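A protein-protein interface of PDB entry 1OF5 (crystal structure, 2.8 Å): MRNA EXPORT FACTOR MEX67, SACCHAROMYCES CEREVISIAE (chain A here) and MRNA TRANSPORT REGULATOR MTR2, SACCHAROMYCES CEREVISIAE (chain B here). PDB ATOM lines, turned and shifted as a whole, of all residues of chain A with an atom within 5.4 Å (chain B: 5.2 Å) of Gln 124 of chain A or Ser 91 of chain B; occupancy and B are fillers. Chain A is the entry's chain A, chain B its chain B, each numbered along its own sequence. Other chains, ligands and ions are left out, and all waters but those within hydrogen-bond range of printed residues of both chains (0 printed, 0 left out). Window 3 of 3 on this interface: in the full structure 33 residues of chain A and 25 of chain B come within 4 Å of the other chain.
The side-chain hydroxyl of Tyr 122 of chain A is in hydrogen-bond range of the side-chain hydroxyl of Thr 93 of chain B, 3.1 Å away.
The side-chain hydroxyl of Ser 167 of chain B sits at hydrogen-bond distance from the side-chain amide nitrogen of Gln 124 of chain A (3.3 Å).
The backbone carbonyl oxygen (O) of Ser 167 of chain B is in hydrogen-bond range of the guanidinium group (NH1) of Arg 51 of chain B, 3.1 Å away.
OG of Ser 91 of chain B sits at hydrogen-bond distance from O of Ile 88 of chain B (2.5 Å).
O of Thr 93 of chain B is in hydrogen-bond range of N of Ile 88 of chain B.
The side-chain hydroxyl (OG) of Ser 91 of chain B is in hydrogen-bond range of the backbone NH (N) of Thr 93 of chain B, at 2.8 Å.
O of Ile 152 of chain B sits at hydrogen-bond distance from N of Ser 167 of chain B (3.1 Å).
Among the printed residues, merely in contact across the chains: Ile 125 of chain A with Ser 91 of chain B (3.2 Å), Tyr 122 of chain A with Ile 152 of chain B (3.4 Å), Pro 123 of chain A with Arg 51 of chain B (3.5 Å), Tyr 122 of chain A with Ile 88 of chain B (3.8 Å), Tyr 122 of chain A with Leu 94 of chain B (3.9 Å) and Gln 124 of chain A with Ser 91 of chain B (3.9 Å).
Of chain B, only Ser 91 (3.9 Å) and Ser 167 (3.3 Å) come within 4 Å of Gln 124 of chain A.
Of chain A, only Gln 124 (3.9 Å) and Ile 125 (3.2 Å) come within 4 Å of Ser 91 of chain B.
Printed residues of chain A within 4 Å of Thr 93 of chain B: Tyr 122.
Printed residues of chain B within 4 Å of Pro 123 of chain A: Arg 51.
Of the printed residues of chain B, Ile 125 of chain A touches Ser 91.
Printed residues of chain B within 4 Å of Tyr 122 of chain A: Ile 88, Thr 93, Leu 94 and Ile 152.
Gly 92 of chain B touches none of the printed residues of chain A.
The nearest residue of chain B that does not touch Gln 124 of chain A is Thr 93 of chain B (4.1 Å).
The nearest printed residue of chain B that does not touch Ile 125 of chain A is Ile 88 of chain B (4.02 Å).
Printed residues of chain A that touch a printed residue of chain B: Tyr 122, Pro 123, Gln 124 and Ile 125.
Hydrophobic or aromatic side chains of chain A that line the printed part of chain B: Tyr 122, Pro 123 and Ile 125.
Hydrophobic or aromatic side chains of chain B that line the printed part of chain A: Ile 88 and Ile 152.
Among the printed residues, no Asp or Glu carboxylate lies within 4 Å of a Lys or Arg side-chain nitrogen of the other chain.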
ATOM      1  N   TYR A 122      31.974 -17.783  16.590  1.00  0.00           N
ATOM      2  CA  TYR A 122      30.915 -17.374  17.489  1.00  0.00           C
ATOM      3  C   TYR A 122      30.408 -18.708  18.016  1.00  0.00           C
ATOM      4  O   TYR A 122      29.358 -19.212  17.608  1.00  0.00           O
ATOM      5  CB  TYR A 122      29.835 -16.621  16.726  1.00  0.00           C
ATOM      6  CG  TYR A 122      29.051 -15.670  17.591  1.00  0.00           C
ATOM      7  CD1 TYR A 122      28.440 -14.549  17.036  1.00  0.00           C
ATOM      8  CD2 TYR A 122      28.888 -15.908  18.956  1.00  0.00           C
ATOM      9  CE1 TYR A 122      27.679 -13.686  17.814  1.00  0.00           C
ATOM     10  CE2 TYR A 122      28.131 -15.058  19.743  1.00  0.00           C
ATOM     11  CZ  TYR A 122      27.519 -13.946  19.166  1.00  0.00           C
ATOM     12  OH  TYR A 122      26.694 -13.133  19.924  1.00  0.00           O
ATOM     13  N   PRO A 123      31.193 -19.307  18.924  1.00  0.00           N
ATOM     14  CA  PRO A 123      30.936 -20.593  19.570  1.00  0.00           C
ATOM     15  C   PRO A 123      29.494 -20.757  20.003  1.00  0.00           C
ATOM     16  O   PRO A 123      28.853 -21.762  19.688  1.00  0.00           O
ATOM     17  CB  PRO A 123      31.887 -20.570  20.763  1.00  0.00           C
ATOM     18  CG  PRO A 123      33.020 -19.750  20.273  1.00  0.00           C
ATOM     19  CD  PRO A 123      32.323 -18.618  19.575  1.00  0.00           C
ATOM     20  N   GLN A 124      28.993 -19.756  20.717  1.00  0.00           N
ATOM     21  CA  GLN A 124      27.644 -19.767  21.257  1.00  0.00           C
ATOM     22  C   GLN A 124      26.506 -20.040  20.292  1.00  0.00           C
ATOM     23  O   GLN A 124      25.423 -20.434  20.721  1.00  0.00           O
ATOM     24  CB  GLN A 124      27.388 -18.464  22.004  1.00  0.00           C
ATOM     25  CG  GLN A 124      28.367 -18.234  23.141  1.00  0.00           C
ATOM     26  CD  GLN A 124      29.589 -17.420  22.729  1.00  0.00           C
ATOM     27  OE1 GLN A 124      30.217 -17.664  21.688  1.00  0.00           O
ATOM     28  NE2 GLN A 124      29.936 -16.446  23.557  1.00  0.00           N
ATOM     29  N   ILE A 125      26.725 -19.830  19.002  1.00  0.00           N
ATOM     30  CA  ILE A 125      25.677 -20.105  18.021  1.00  0.00           C
ATOM     31  C   ILE A 125      26.250 -20.949  16.910  1.00  0.00           C
ATOM     32  O   ILE A 125      25.725 -20.950  15.788  1.00  0.00           O
ATOM     33  CB  ILE A 125      25.153 -18.845  17.372  1.00  0.00           C
ATOM     34  CG1 ILE A 125      26.305 -18.136  16.654  1.00  0.00           C
ATOM     35  CG2 ILE A 125      24.462 -17.985  18.405  1.00  0.00           C
ATOM     36  CD1 ILE A 125      25.971 -16.743  16.178  1.00  0.00           C
ATOM     37  N   ASN A 126      27.336 -21.651  17.230  1.00  0.00           N
ATOM     38  CA  ASN A 126      28.014 -22.506  16.271  1.00  0.00           C
ATOM     39  C   ASN A 126      28.075 -21.731  14.949  1.00  0.00           C
ATOM     40  O   ASN A 126      27.687 -22.228  13.888  1.00  0.00           O
ATOM     41  CB  ASN A 126      27.233 -23.825  16.134  1.00  0.00           C
ATOM     42  CG  ASN A 126      27.997 -24.880  15.365  1.00  0.00           C
ATOM     43  OD1 ASN A 126      28.285 -24.703  14.173  1.00  0.00           O
ATOM     44  ND2 ASN A 126      28.336 -25.989  16.036  1.00  0.00           N
ATOM     45  N   ARG B  51      38.429 -14.891  22.068  1.00  0.00           N
ATOM     46  CA  ARG B  51      38.641 -14.615  20.674  1.00  0.00           C
ATOM     47  C   ARG B  51      38.855 -13.108  20.687  1.00  0.00           C
ATOM     48  O   ARG B  51      37.934 -12.333  20.954  1.00  0.00           O
ATOM     49  CB  ARG B  51      37.420 -15.023  19.867  1.00  0.00           C
ATOM     50  CG  ARG B  51      37.580 -16.394  19.258  1.00  0.00           C
ATOM     51  CD  ARG B  51      36.326 -17.248  19.387  1.00  0.00           C
ATOM     52  NE  ARG B  51      36.263 -17.993  20.645  1.00  0.00           N
ATOM     53  CZ  ARG B  51      35.491 -17.661  21.672  1.00  0.00           C
ATOM     54  NH1 ARG B  51      34.704 -16.590  21.602  1.00  0.00           N
ATOM     55  NH2 ARG B  51      35.504 -18.402  22.770  1.00  0.00           N
ATOM     56  N   ILE B  88      21.471 -11.776  20.206  1.00  0.00           N
ATOM     57  CA  ILE B  88      21.141 -12.959  19.442  1.00  0.00           C
ATOM     58  C   ILE B  88      20.499 -14.059  20.280  1.00  0.00           C
ATOM     59  O   ILE B  88      21.095 -14.527  21.252  1.00  0.00           O
ATOM     60  CB  ILE B  88      22.401 -13.486  18.721  1.00  0.00           C
ATOM     61  CG1 ILE B  88      22.922 -12.406  17.762  1.00  0.00           C
ATOM     62  CG2 ILE B  88      22.081 -14.775  17.971  1.00  0.00           C
ATOM     63  CD1 ILE B  88      24.075 -12.844  16.885  1.00  0.00           C
ATOM     64  N   PRO B  89      19.236 -14.409  19.960  1.00  0.00           N
ATOM     65  CA  PRO B  89      18.283 -15.380  20.475  1.00  0.00           C
ATOM     66  C   PRO B  89      18.784 -16.796  20.624  1.00  0.00           C
ATOM     67  O   PRO B  89      18.940 -17.482  19.631  1.00  0.00           O
ATOM     68  CB  PRO B  89      17.154 -15.303  19.458  1.00  0.00           C
ATOM     69  CG  PRO B  89      17.091 -13.888  19.157  1.00  0.00           C
ATOM     70  CD  PRO B  89      18.540 -13.444  19.081  1.00  0.00           C
ATOM     71  N   GLY B  90      18.928 -17.252  21.867  1.00  0.00           N
ATOM     72  CA  GLY B  90      19.381 -18.606  22.112  1.00  0.00           C
ATOM     73  C   GLY B  90      20.859 -18.579  22.418  1.00  0.00           C
ATOM     74  O   GLY B  90      21.346 -19.306  23.304  1.00  0.00           O
ATOM     75  N   SER B  91      21.574 -17.719  21.695  1.00  0.00           N
ATOM     76  CA  SER B  91      23.007 -17.582  21.891  1.00  0.00           C
ATOM     77  C   SER B  91      23.225 -17.282  23.364  1.00  0.00           C
ATOM     78  O   SER B  91      24.102 -17.870  24.011  1.00  0.00           O
ATOM     79  CB  SER B  91      23.559 -16.422  21.053  1.00  0.00           C
ATOM     80  OG  SER B  91      23.438 -15.157  21.712  1.00  0.00           O
ATOM     81  N   GLY B  92      22.408 -16.375  23.895  1.00  0.00           N
ATOM     82  CA  GLY B  92      22.544 -15.998  25.291  1.00  0.00           C
ATOM     83  C   GLY B  92      23.542 -14.866  25.417  1.00  0.00           C
ATOM     84  O   GLY B  92      24.141 -14.648  26.477  1.00  0.00           O
ATOM     85  N   THR B  93      23.707 -14.135  24.318  1.00  0.00           N
ATOM     86  CA  THR B  93      24.643 -13.027  24.270  1.00  0.00           C
ATOM     87  C   THR B  93      24.206 -12.023  23.237  1.00  0.00           C
ATOM     88  O   THR B  93      23.193 -12.195  22.564  1.00  0.00           O
ATOM     89  CB  THR B  93      26.067 -13.496  23.885  1.00  0.00           C
ATOM     90  OG1 THR B  93      26.001 -14.273  22.679  1.00  0.00           O
ATOM     91  CG2 THR B  93      26.698 -14.326  25.013  1.00  0.00           C
ATOM     92  N   LEU B  94      25.004 -10.976  23.107  1.00  0.00           N
ATOM     93  CA  LEU B  94      24.736  -9.913  22.167  1.00  0.00           C
ATOM     94  C   LEU B  94      26.046  -9.484  21.500  1.00  0.00           C
ATOM     95  O   LEU B  94      27.144  -9.842  21.941  1.00  0.00           O
ATOM     96  CB  LEU B  94      24.114  -8.742  22.911  1.00  0.00           C
ATOM     97  CG  LEU B  94      25.078  -7.997  23.830  1.00  0.00           C
ATOM     98  CD1 LEU B  94      25.326  -6.618  23.215  1.00  0.00           C
ATOM     99  CD2 LEU B  94      24.515  -7.877  25.242  1.00  0.00           C
ATOM    100  N   ILE B 152      31.440  -9.307  21.609  1.00  0.00           N
ATOM    101  CA  ILE B 152      30.390 -10.284  21.856  1.00  0.00           C
ATOM    102  C   ILE B 152      30.313 -10.272  23.365  1.00  0.00           C
ATOM    103  O   ILE B 152      31.321 -10.497  24.042  1.00  0.00           O
ATOM    104  CB  ILE B 152      30.764 -11.680  21.328  1.00  0.00           C
ATOM    105  CG1 ILE B 152      30.986 -11.594  19.810  1.00  0.00           C
ATOM    106  CG2 ILE B 152      29.654 -12.666  21.645  1.00  0.00           C
ATOM    107  CD1 ILE B 152      31.200 -12.901  19.122  1.00  0.00           C
ATOM    108  N   SER B 167      33.634 -12.116  25.221  1.00  0.00           N
ATOM    109  CA  SER B 167      34.165 -13.318  24.581  1.00  0.00           C
ATOM    110  C   SER B 167      34.600 -12.947  23.177  1.00  0.00           C
ATOM    111  O   SER B 167      35.298 -13.712  22.509  1.00  0.00           O
ATOM    112  CB  SER B 167      33.107 -14.428  24.528  1.00  0.00           C
ATOM    113  OG  SER B 167      31.782 -13.910  24.571  1.00  0.00           O
